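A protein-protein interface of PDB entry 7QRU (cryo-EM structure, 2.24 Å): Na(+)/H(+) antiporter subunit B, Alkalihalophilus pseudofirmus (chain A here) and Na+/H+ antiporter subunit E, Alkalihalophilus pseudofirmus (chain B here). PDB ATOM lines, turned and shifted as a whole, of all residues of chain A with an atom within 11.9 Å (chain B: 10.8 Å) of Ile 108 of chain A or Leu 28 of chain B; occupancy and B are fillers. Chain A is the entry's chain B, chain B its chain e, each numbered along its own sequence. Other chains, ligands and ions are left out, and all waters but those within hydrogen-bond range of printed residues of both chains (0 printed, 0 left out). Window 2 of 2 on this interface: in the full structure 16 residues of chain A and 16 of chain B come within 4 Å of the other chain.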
ATOM      1  N   VAL A  27       5.999 -14.667 -24.612  1.00  0.00           N
ATOM      2  CA  VAL A  27       6.538 -14.157 -23.367  1.00  0.00           C
ATOM      3  C   VAL A  27       8.050 -14.027 -23.467  1.00  0.00           C
ATOM      4  O   VAL A  27       8.586 -13.102 -22.928  1.00  0.00           O
ATOM      5  CB  VAL A  27       6.123 -15.029 -22.170  1.00  0.00           C
ATOM      6  CG1 VAL A  27       6.805 -14.596 -20.907  1.00  0.00           C
ATOM      7  CG2 VAL A  27       4.639 -15.062 -22.077  1.00  0.00           C
ATOM      8  N   PHE A  31      10.220 -10.511 -22.744  1.00  0.00           N
ATOM      9  CA  PHE A  31      11.293 -10.261 -21.800  1.00  0.00           C
ATOM     10  C   PHE A  31      12.636 -10.055 -22.487  1.00  0.00           C
ATOM     11  O   PHE A  31      13.570  -9.751 -21.836  1.00  0.00           O
ATOM     12  CB  PHE A  31      11.433 -11.427 -20.831  1.00  0.00           C
ATOM     13  CG  PHE A  31      10.403 -11.364 -19.761  1.00  0.00           C
ATOM     14  CD1 PHE A  31      10.501 -10.410 -18.774  1.00  0.00           C
ATOM     15  CD2 PHE A  31       9.262 -12.139 -19.831  1.00  0.00           C
ATOM     16  CE1 PHE A  31       9.522 -10.327 -17.797  1.00  0.00           C
ATOM     17  CE2 PHE A  31       8.276 -12.052 -18.866  1.00  0.00           C
ATOM     18  CZ  PHE A  31       8.409 -11.140 -17.856  1.00  0.00           C
ATOM     19  N   TYR A 104      20.687  -5.671  -8.623  1.00  0.00           N
ATOM     20  CA  TYR A 104      20.521  -6.210  -7.263  1.00  0.00           C
ATOM     21  C   TYR A 104      21.096  -7.635  -7.155  1.00  0.00           C
ATOM     22  O   TYR A 104      21.397  -8.247  -8.169  1.00  0.00           O
ATOM     23  CB  TYR A 104      19.050  -6.228  -6.839  1.00  0.00           C
ATOM     24  CG  TYR A 104      18.421  -4.858  -6.785  1.00  0.00           C
ATOM     25  CD1 TYR A 104      17.876  -4.281  -7.919  1.00  0.00           C
ATOM     26  CD2 TYR A 104      18.439  -4.097  -5.627  1.00  0.00           C
ATOM     27  CE1 TYR A 104      17.320  -3.011  -7.894  1.00  0.00           C
ATOM     28  CE2 TYR A 104      17.884  -2.826  -5.581  1.00  0.00           C
ATOM     29  CZ  TYR A 104      17.327  -2.273  -6.721  1.00  0.00           C
ATOM     30  OH  TYR A 104      16.766  -1.011  -6.676  1.00  0.00           O
ATOM     31  N   GLN A 105      21.290  -8.156  -5.921  1.00  0.00           N
ATOM     32  CA  GLN A 105      21.620  -9.566  -5.684  1.00  0.00           C
ATOM     33  C   GLN A 105      20.490 -10.213  -4.899  1.00  0.00           C
ATOM     34  O   GLN A 105      20.124  -9.724  -3.831  1.00  0.00           O
ATOM     35  CB  GLN A 105      22.880  -9.787  -4.845  1.00  0.00           C
ATOM     36  CG  GLN A 105      24.002  -8.797  -5.121  1.00  0.00           C
ATOM     37  CD  GLN A 105      24.601  -8.967  -6.493  1.00  0.00           C
ATOM     38  OE1 GLN A 105      24.671  -8.018  -7.277  1.00  0.00           O
ATOM     39  NE2 GLN A 105      25.044 -10.183  -6.774  1.00  0.00           N
ATOM     40  N   ILE A 106      19.904 -11.264  -5.473  1.00  0.00           N
ATOM     41  CA  ILE A 106      18.979 -12.109  -4.759  1.00  0.00           C
ATOM     42  C   ILE A 106      19.706 -13.425  -4.574  1.00  0.00           C
ATOM     43  O   ILE A 106      20.224 -13.948  -5.556  1.00  0.00           O
ATOM     44  CB  ILE A 106      17.676 -12.269  -5.554  1.00  0.00           C
ATOM     45  CG1 ILE A 106      16.957 -10.930  -5.695  1.00  0.00           C
ATOM     46  CG2 ILE A 106      16.809 -13.337  -4.912  1.00  0.00           C
ATOM     47  CD1 ILE A 106      15.637 -11.018  -6.420  1.00  0.00           C
ATOM     48  N   PRO A 107      19.818 -13.968  -3.336  1.00  0.00           N
ATOM     49  CA  PRO A 107      20.294 -15.346  -3.148  1.00  0.00           C
ATOM     50  C   PRO A 107      19.630 -16.414  -4.034  1.00  0.00           C
ATOM     51  O   PRO A 107      20.331 -17.155  -4.724  1.00  0.00           O
ATOM     52  CB  PRO A 107      19.956 -15.643  -1.677  1.00  0.00           C
ATOM     53  CG  PRO A 107      19.960 -14.284  -1.001  1.00  0.00           C
ATOM     54  CD  PRO A 107      19.525 -13.289  -2.060  1.00  0.00           C
ATOM     55  N   ILE A 108      18.278 -16.473  -4.012  1.00  0.00           N
ATOM     56  CA  ILE A 108      17.476 -17.492  -4.698  1.00  0.00           C
ATOM     57  C   ILE A 108      17.905 -17.583  -6.153  1.00  0.00           C
ATOM     58  O   ILE A 108      18.324 -18.637  -6.620  1.00  0.00           O
ATOM     59  CB  ILE A 108      15.950 -17.218  -4.689  1.00  0.00           C
ATOM     60  CG1 ILE A 108      15.476 -16.389  -3.491  1.00  0.00           C
ATOM     61  CG2 ILE A 108      15.187 -18.531  -4.827  1.00  0.00           C
ATOM     62  CD1 ILE A 108      14.006 -16.013  -3.534  1.00  0.00           C
ATOM     63  N   LEU A 109      17.728 -16.464  -6.858  1.00  0.00           N
ATOM     64  CA  LEU A 109      18.066 -16.371  -8.271  1.00  0.00           C
ATOM     65  C   LEU A 109      19.579 -16.180  -8.423  1.00  0.00           C
ATOM     66  O   LEU A 109      20.316 -17.145  -8.637  1.00  0.00           O
ATOM     67  CB  LEU A 109      17.274 -15.218  -8.900  1.00  0.00           C
ATOM     68  CG  LEU A 109      15.761 -15.417  -8.975  1.00  0.00           C
ATOM     69  CD1 LEU A 109      15.041 -14.847  -7.761  1.00  0.00           C
ATOM     70  CD2 LEU A 109      15.196 -14.779 -10.225  1.00  0.00           C
ATOM     71  N   GLY A 110      20.035 -14.932  -8.268  1.00  0.00           N
ATOM     72  CA  GLY A 110      21.412 -14.523  -8.491  1.00  0.00           C
ATOM     73  C   GLY A 110      21.454 -13.024  -8.768  1.00  0.00           C
ATOM     74  O   GLY A 110      20.502 -12.322  -8.432  1.00  0.00           O
ATOM     75  N   GLU A 111      22.547 -12.536  -9.371  1.00  0.00           N
ATOM     76  CA  GLU A 111      22.596 -11.152  -9.824  1.00  0.00           C
ATOM     77  C   GLU A 111      21.452 -10.944 -10.807  1.00  0.00           C
ATOM     78  O   GLU A 111      21.317 -11.733 -11.733  1.00  0.00           O
ATOM     79  CB  GLU A 111      23.919 -10.818 -10.515  1.00  0.00           C
ATOM     80  CG  GLU A 111      24.026  -9.356 -10.930  1.00  0.00           C
ATOM     81  CD  GLU A 111      25.229  -9.012 -11.792  1.00  0.00           C
ATOM     82  OE1 GLU A 111      25.843  -9.949 -12.342  1.00  0.00           O
ATOM     83  OE2 GLU A 111      25.570  -7.814 -11.906  1.00  0.00           O
ATOM     84  N   THR A 112      20.626  -9.915 -10.589  1.00  0.00           N
ATOM     85  CA  THR A 112      19.478  -9.657 -11.451  1.00  0.00           C
ATOM     86  C   THR A 112      19.378  -8.152 -11.735  1.00  0.00           C
ATOM     87  O   THR A 112      19.569  -7.327 -10.844  1.00  0.00           O
ATOM     88  CB  THR A 112      18.200 -10.215 -10.818  1.00  0.00           C
ATOM     89  OG1 THR A 112      17.086  -9.718 -11.555  1.00  0.00           O
ATOM     90  CG2 THR A 112      18.059  -9.815  -9.365  1.00  0.00           C
ATOM     91  N   ASN B   8       5.190 -27.995 -17.555  1.00  0.00           N
ATOM     92  CA  ASN B   8       5.815 -26.813 -17.041  1.00  0.00           C
ATOM     93  C   ASN B   8       7.310 -26.956 -17.198  1.00  0.00           C
ATOM     94  O   ASN B   8       8.005 -25.989 -17.440  1.00  0.00           O
ATOM     95  CB  ASN B   8       5.424 -26.660 -15.568  1.00  0.00           C
ATOM     96  CG  ASN B   8       5.112 -25.276 -15.114  1.00  0.00           C
ATOM     97  OD1 ASN B   8       5.738 -24.318 -15.523  1.00  0.00           O
ATOM     98  ND2 ASN B   8       4.152 -25.209 -14.186  1.00  0.00           N
ATOM     99  N   LEU B   9       7.887 -28.147 -16.909  1.00  0.00           N
ATOM    100  CA  LEU B   9       9.323 -28.375 -17.107  1.00  0.00           C
ATOM    101  C   LEU B   9       9.688 -28.383 -18.597  1.00  0.00           C
ATOM    102  O   LEU B   9      10.717 -27.822 -18.957  1.00  0.00           O
ATOM    103  CB  LEU B   9       9.676 -29.734 -16.497  1.00  0.00           C
ATOM    104  CG  LEU B   9       9.737 -29.798 -14.983  1.00  0.00           C
ATOM    105  CD1 LEU B   9       9.750 -31.239 -14.623  1.00  0.00           C
ATOM    106  CD2 LEU B   9      10.951 -29.051 -14.439  1.00  0.00           C
ATOM    107  N   ILE B  11       8.095 -26.466 -20.836  1.00  0.00           N
ATOM    108  CA  ILE B  11       8.166 -25.058 -21.095  1.00  0.00           C
ATOM    109  C   ILE B  11       9.523 -24.524 -20.656  1.00  0.00           C
ATOM    110  O   ILE B  11      10.136 -23.644 -21.314  1.00  0.00           O
ATOM    111  CB  ILE B  11       7.042 -24.212 -20.478  1.00  0.00           C
ATOM    112  CG1 ILE B  11       5.662 -24.468 -21.062  1.00  0.00           C
ATOM    113  CG2 ILE B  11       7.422 -22.704 -20.539  1.00  0.00           C
ATOM    114  CD1 ILE B  11       5.610 -24.196 -22.515  1.00  0.00           C
ATOM    115  N   ALA B  12      10.009 -25.002 -19.547  1.00  0.00           N
ATOM    116  CA  ALA B  12      11.269 -24.475 -19.035  1.00  0.00           C
ATOM    117  C   ALA B  12      12.418 -25.011 -19.908  1.00  0.00           C
ATOM    118  O   ALA B  12      13.438 -24.333 -20.063  1.00  0.00           O
ATOM    119  CB  ALA B  12      11.423 -24.817 -17.585  1.00  0.00           C
ATOM    120  N   VAL B  13      12.212 -26.196 -20.535  1.00  0.00           N
ATOM    121  CA  VAL B  13      13.215 -26.740 -21.469  1.00  0.00           C
ATOM    122  C   VAL B  13      13.250 -25.850 -22.720  1.00  0.00           C
ATOM    123  O   VAL B  13      14.353 -25.466 -23.136  1.00  0.00           O
ATOM    124  CB  VAL B  13      12.927 -28.234 -21.816  1.00  0.00           C
ATOM    125  CG1 VAL B  13      13.585 -28.741 -23.093  1.00  0.00           C
ATOM    126  CG2 VAL B  13      13.240 -29.161 -20.662  1.00  0.00           C
ATOM    127  N   TRP B  15      12.290 -22.805 -22.742  1.00  0.00           N
ATOM    128  CA  TRP B  15      12.698 -21.506 -22.263  1.00  0.00           C
ATOM    129  C   TRP B  15      14.181 -21.352 -22.112  1.00  0.00           C
ATOM    130  O   TRP B  15      14.758 -20.239 -22.328  1.00  0.00           O
ATOM    131  CB  TRP B  15      11.970 -21.109 -20.935  1.00  0.00           C
ATOM    132  CG  TRP B  15      12.343 -19.784 -20.329  1.00  0.00           C
ATOM    133  CD1 TRP B  15      13.435 -19.514 -19.610  1.00  0.00           C
ATOM    134  CD2 TRP B  15      11.709 -18.485 -20.555  1.00  0.00           C
ATOM    135  NE1 TRP B  15      13.510 -18.161 -19.215  1.00  0.00           N
ATOM    136  CE2 TRP B  15      12.497 -17.511 -19.886  1.00  0.00           C
ATOM    137  CE3 TRP B  15      10.541 -18.116 -21.241  1.00  0.00           C
ATOM    138  CZ2 TRP B  15      12.129 -16.170 -19.888  1.00  0.00           C
ATOM    139  CZ3 TRP B  15      10.239 -16.777 -21.281  1.00  0.00           C
ATOM    140  CH2 TRP B  15      10.958 -15.851 -20.555  1.00  0.00           C
ATOM    141  N   VAL B  16      14.823 -22.372 -21.550  1.00  0.00           N
ATOM    142  CA  VAL B  16      16.127 -22.074 -20.918  1.00  0.00           C
ATOM    143  C   VAL B  16      17.204 -21.773 -21.970  1.00  0.00           C
ATOM    144  O   VAL B  16      18.049 -20.856 -21.806  1.00  0.00           O
ATOM    145  CB  VAL B  16      16.537 -23.223 -19.989  1.00  0.00           C
ATOM    146  CG1 VAL B  16      16.529 -24.539 -20.816  1.00  0.00           C
ATOM    147  CG2 VAL B  16      17.793 -22.806 -19.242  1.00  0.00           C
ATOM    148  N   GLN B  19      17.419 -18.108 -23.604  1.00  0.00           N
ATOM    149  CA  GLN B  19      18.223 -17.103 -22.891  1.00  0.00           C
ATOM    150  C   GLN B  19      19.697 -17.514 -22.910  1.00  0.00           C
ATOM    151  O   GLN B  19      20.582 -16.657 -22.908  1.00  0.00           O
ATOM    152  CB  GLN B  19      17.746 -17.006 -21.438  1.00  0.00           C
ATOM    153  CG  GLN B  19      16.279 -17.344 -21.315  1.00  0.00           C
ATOM    154  CD  GLN B  19      15.539 -16.081 -21.634  1.00  0.00           C
ATOM    155  OE1 GLN B  19      14.359 -16.177 -21.981  1.00  0.00           O
ATOM    156  NE2 GLN B  19      16.200 -14.943 -21.416  1.00  0.00           N
ATOM    157  N   SER B  21      21.271 -18.558 -20.467  1.00  0.00           N
ATOM    158  CA  SER B  21      21.893 -18.145 -19.218  1.00  0.00           C
ATOM    159  C   SER B  21      22.372 -19.346 -18.394  1.00  0.00           C
ATOM    160  O   SER B  21      23.497 -19.297 -17.874  1.00  0.00           O
ATOM    161  CB  SER B  21      20.983 -17.267 -18.415  1.00  0.00           C
ATOM    162  OG  SER B  21      20.701 -16.050 -19.107  1.00  0.00           O
ATOM    163  N   TYR B  22      21.540 -20.399 -18.273  1.00  0.00           N
ATOM    164  CA  TYR B  22      21.830 -21.564 -17.429  1.00  0.00           C
ATOM    165  C   TYR B  22      22.210 -21.159 -16.004  1.00  0.00           C
ATOM    166  O   TYR B  22      23.161 -21.673 -15.425  1.00  0.00           O
ATOM    167  CB  TYR B  22      22.920 -22.380 -18.115  1.00  0.00           C
ATOM    168  CG  TYR B  22      22.549 -22.784 -19.514  1.00  0.00           C
ATOM    169  CD1 TYR B  22      21.433 -23.568 -19.702  1.00  0.00           C
ATOM    170  CD2 TYR B  22      23.342 -22.460 -20.612  1.00  0.00           C
ATOM    171  CE1 TYR B  22      21.148 -24.082 -20.961  1.00  0.00           C
ATOM    172  CE2 TYR B  22      22.984 -22.835 -21.891  1.00  0.00           C
ATOM    173  CZ  TYR B  22      21.886 -23.659 -22.054  1.00  0.00           C
ATOM    174  OH  TYR B  22      21.548 -24.107 -23.282  1.00  0.00           O
ATOM    175  N   THR B  23      21.444 -20.209 -15.455  1.00  0.00           N
ATOM    176  CA  THR B  23      21.554 -19.747 -14.083  1.00  0.00           C
ATOM    177  C   THR B  23      20.272 -20.093 -13.332  1.00  0.00           C
ATOM    178  O   THR B  23      19.272 -20.414 -13.951  1.00  0.00           O
ATOM    179  CB  THR B  23      21.774 -18.236 -14.048  1.00  0.00           C
ATOM    180  OG1 THR B  23      20.691 -17.600 -14.715  1.00  0.00           O
ATOM    181  CG2 THR B  23      23.057 -17.828 -14.733  1.00  0.00           C
ATOM    182  N   ALA B  24      20.287 -20.024 -12.002  1.00  0.00           N
ATOM    183  CA  ALA B  24      19.063 -20.239 -11.251  1.00  0.00           C
ATOM    184  C   ALA B  24      18.065 -19.140 -11.584  1.00  0.00           C
ATOM    185  O   ALA B  24      16.870 -19.411 -11.661  1.00  0.00           O
ATOM    186  CB  ALA B  24      19.361 -20.290  -9.764  1.00  0.00           C
ATOM    187  N   VAL B  25      18.552 -17.922 -11.803  1.00  0.00           N
ATOM    188  CA  VAL B  25      17.704 -16.769 -12.081  1.00  0.00           C
ATOM    189  C   VAL B  25      16.835 -17.093 -13.293  1.00  0.00           C
ATOM    190  O   VAL B  25      15.622 -16.975 -13.231  1.00  0.00           O
ATOM    191  CB  VAL B  25      18.527 -15.494 -12.379  1.00  0.00           C
ATOM    192  CG1 VAL B  25      17.755 -14.191 -12.174  1.00  0.00           C
ATOM    193  CG2 VAL B  25      19.844 -15.487 -11.626  1.00  0.00           C
ATOM    194  N   ASP B  26      17.442 -17.512 -14.413  1.00  0.00           N
ATOM    195  CA  ASP B  26      16.676 -17.751 -15.633  1.00  0.00           C
ATOM    196  C   ASP B  26      15.835 -19.031 -15.537  1.00  0.00           C
ATOM    197  O   ASP B  26      14.708 -18.998 -16.025  1.00  0.00           O
ATOM    198  CB  ASP B  26      17.569 -17.703 -16.877  1.00  0.00           C
ATOM    199  CG  ASP B  26      17.987 -16.275 -17.206  1.00  0.00           C
ATOM    200  OD1 ASP B  26      18.616 -15.657 -16.304  1.00  0.00           O
ATOM    201  OD2 ASP B  26      17.652 -15.775 -18.345  1.00  0.00           O
ATOM    202  N   PHE B  27      16.299 -20.106 -14.865  1.00  0.00           N
ATOM    203  CA  PHE B  27      15.435 -21.275 -14.799  1.00  0.00           C
ATOM    204  C   PHE B  27      14.198 -20.988 -13.922  1.00  0.00           C
ATOM    205  O   PHE B  27      13.073 -21.431 -14.153  1.00  0.00           O
ATOM    206  CB  PHE B  27      16.100 -22.515 -14.223  1.00  0.00           C
ATOM    207  CG  PHE B  27      15.315 -23.786 -14.527  1.00  0.00           C
ATOM    208  CD1 PHE B  27      15.547 -24.445 -15.698  1.00  0.00           C
ATOM    209  CD2 PHE B  27      14.513 -24.433 -13.603  1.00  0.00           C
ATOM    210  CE1 PHE B  27      14.996 -25.697 -15.987  1.00  0.00           C
ATOM    211  CE2 PHE B  27      13.919 -25.659 -13.886  1.00  0.00           C
ATOM    212  CZ  PHE B  27      14.197 -26.330 -15.062  1.00  0.00           C
ATOM    213  N   LEU B  28      14.371 -20.197 -12.878  1.00  0.00           N
ATOM    214  CA  LEU B  28      13.234 -19.889 -12.028  1.00  0.00           C
ATOM    215  C   LEU B  28      12.277 -19.003 -12.812  1.00  0.00           C
ATOM    216  O   LEU B  28      11.076 -19.169 -12.667  1.00  0.00           O
ATOM    217  CB  LEU B  28      13.694 -19.231 -10.719  1.00  0.00           C
ATOM    218  CG  LEU B  28      14.258 -20.262  -9.743  1.00  0.00           C
ATOM    219  CD1 LEU B  28      14.796 -19.575  -8.495  1.00  0.00           C
ATOM    220  CD2 LEU B  28      13.216 -21.332  -9.424  1.00  0.00           C
ATOM    221  N   ILE B  29      12.786 -18.053 -13.611  1.00  0.00           N
ATOM    222  CA  ILE B  29      11.905 -17.311 -14.513  1.00  0.00           C
ATOM    223  C   ILE B  29      11.183 -18.254 -15.488  1.00  0.00           C
ATOM    224  O   ILE B  29       9.968 -18.169 -15.664  1.00  0.00           O
ATOM    225  CB  ILE B  29      12.636 -16.191 -15.238  1.00  0.00           C
ATOM    226  CG1 ILE B  29      13.208 -15.197 -14.222  1.00  0.00           C
ATOM    227  CG2 ILE B  29      11.692 -15.499 -16.231  1.00  0.00           C
ATOM    228  CD1 ILE B  29      14.083 -14.081 -14.813  1.00  0.00           C
ATOM    229  N   GLY B  30      11.881 -19.259 -15.932  1.00  0.00           N
ATOM    230  CA  GLY B  30      11.355 -20.174 -16.906  1.00  0.00           C
ATOM    231  C   GLY B  30      10.281 -21.067 -16.367  1.00  0.00           C
ATOM    232  O   GLY B  30       9.405 -21.516 -17.117  1.00  0.00           O
ATOM    233  N   TYR B  31      10.371 -21.460 -15.079  1.00  0.00           N
ATOM    234  CA  TYR B  31       9.451 -22.480 -14.554  1.00  0.00           C
ATOM    235  C   TYR B  31       8.163 -21.733 -14.248  1.00  0.00           C
ATOM    236  O   TYR B  31       7.074 -22.286 -14.499  1.00  0.00           O
ATOM    237  CB  TYR B  31       9.997 -23.245 -13.331  1.00  0.00           C
ATOM    238  CG  TYR B  31       9.035 -24.313 -12.900  1.00  0.00           C
ATOM    239  CD1 TYR B  31       9.069 -25.548 -13.501  1.00  0.00           C
ATOM    240  CD2 TYR B  31       7.994 -24.010 -12.022  1.00  0.00           C
ATOM    241  CE1 TYR B  31       8.097 -26.492 -13.259  1.00  0.00           C
ATOM    242  CE2 TYR B  31       7.019 -24.945 -11.761  1.00  0.00           C
ATOM    243  CZ  TYR B  31       7.089 -26.184 -12.368  1.00  0.00           C
ATOM    244  OH  TYR B  31       6.089 -27.086 -12.138  1.00  0.00           O
ATOM    245  N   VAL B  32       8.323 -20.462 -13.888  1.00  0.00           N
ATOM    246  CA  VAL B  32       7.197 -19.633 -13.530  1.00  0.00           C
ATOM    247  C   VAL B  32       6.429 -19.221 -14.770  1.00  0.00           C
ATOM    248  O   VAL B  32       5.217 -19.285 -14.748  1.00  0.00           O
ATOM    249  CB  VAL B  32       7.720 -18.398 -12.765  1.00  0.00           C
ATOM    250  CG1 VAL B  32       6.682 -17.349 -12.514  1.00  0.00           C
ATOM    251  CG2 VAL B  32       8.234 -18.827 -11.427  1.00  0.00           C
ATOM    252  N   VAL B  33       7.124 -18.774 -15.824  1.00  0.00           N
ATOM    253  CA  VAL B  33       6.508 -18.530 -17.118  1.00  0.00           C
ATOM    254  C   VAL B  33       5.591 -19.680 -17.503  1.00  0.00           C
ATOM    255  O   VAL B  33       4.442 -19.519 -17.865  1.00  0.00           O
ATOM    256  CB  VAL B  33       7.508 -18.295 -18.226  1.00  0.00           C
ATOM    257  CG1 VAL B  33       6.793 -18.389 -19.553  1.00  0.00           C
ATOM    258  CG2 VAL B  33       8.161 -16.921 -18.051  1.00  0.00           C
ATOM    259  N   GLY B  34       6.015 -20.876 -17.355  1.00  0.00           N
ATOM    260  CA  GLY B  34       5.119 -21.954 -17.726  1.00  0.00           C
ATOM    261  C   GLY B  34       3.922 -22.032 -16.826  1.00  0.00           C
ATOM    262  O   GLY B  34       2.889 -22.428 -17.327  1.00  0.00           O
ATOM    263  N   ILE B  35       4.040 -21.661 -15.515  1.00  0.00           N
ATOM    264  CA  ILE B  35       2.869 -21.688 -14.606  1.00  0.00           C
ATOM    265  C   ILE B  35       1.817 -20.711 -15.106  1.00  0.00           C
ATOM    266  O   ILE B  35       0.676 -21.065 -15.226  1.00  0.00           O
ATOM    267  CB  ILE B  35       3.275 -21.332 -13.149  1.00  0.00           C
ATOM    268  CG1 ILE B  35       4.222 -22.388 -12.588  1.00  0.00           C
ATOM    269  CG2 ILE B  35       2.181 -21.145 -12.211  1.00  0.00           C
ATOM    270  CD1 ILE B  35       4.759 -21.919 -11.276  1.00  0.00           C
ATOM    271  N   PHE B  36       2.282 -19.527 -15.512  1.00  0.00           N
ATOM    272  CA  PHE B  36       1.406 -18.491 -15.988  1.00  0.00           C
ATOM    273  C   PHE B  36       0.715 -18.945 -17.283  1.00  0.00           C
ATOM    274  O   PHE B  36      -0.494 -18.753 -17.404  1.00  0.00           O
ATOM    275  CB  PHE B  36       2.202 -17.205 -16.154  1.00  0.00           C
ATOM    276  CG  PHE B  36       1.567 -16.179 -17.063  1.00  0.00           C
ATOM    277  CD1 PHE B  36       0.508 -15.383 -16.598  1.00  0.00           C
ATOM    278  CD2 PHE B  36       2.033 -15.990 -18.367  1.00  0.00           C
ATOM    279  CE1 PHE B  36      -0.079 -14.436 -17.427  1.00  0.00           C
ATOM    280  CE2 PHE B  36       1.418 -15.070 -19.208  1.00  0.00           C
ATOM    281  CZ  PHE B  36       0.374 -14.297 -18.737  1.00  0.00           C
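Among the printed residues, merely in contact across the chains: Val 27 of chain A with Val 33 of chain B, Ile 108 of chain A with Ala 24 of chain B, Ile 108 of chain A with Leu 28 of chain B, Leu 109 of chain A with Ala 24 of chain B, Leu 109 of chain A with Val 25 of chain B and Gly 110 of chain A with Val 25 of chain B.
Ile 108 of chain A touches just these residues of chain B: Ala 24 (3.7 Å) and Leu 28 (3.8 Å).
Leu 28 of chain B touches one residue of chain A.
No residue of chain B comes within 4 Å of Pro 107 of chain A.
Of chain B, only Ala 24 (3.5 Å) and Val 25 (3.3 Å) come within 4 Å of Leu 109 of chain A.
Of chain B, only Val 25 (3.4 Å) comes within 4 Å of Gly 110 of chain A.
Val 25 of chain B touches two residues of chain A.
No residue of chain A comes within 4 Å of Asp 26 of chain B.
No residue of chain A comes within 4 Å of Ile 29 of chain B.
No residue of chain A comes within 4 Å of Gly 30 of chain B.
Of the printed residues of chain B, Val 27 of chain A touches Val 33 (3.9 Å).
Of the printed residues of chain A, Val 33 of chain B touches Val 27 (3.9 Å).
Ala 12 of chain B touches none of the printed residues of chain A.
The nearest residue of chain B that does not touch Ile 108 of chain A is Val 25 of chain B (5.2 Å).
The nearest residue of chain A that does not touch Leu 28 of chain B is Leu 109 of chain A (4.3 Å).
The nearest printed residue of chain B that does not touch Val 27 of chain A is Trp 15 of chain B (4.1 Å).
Of the 24 printed residues of chain B, 4 touch a printed residue of chain A.
Along chain B the printed residues that touch a printed residue of chain A span positions 24 to 33.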
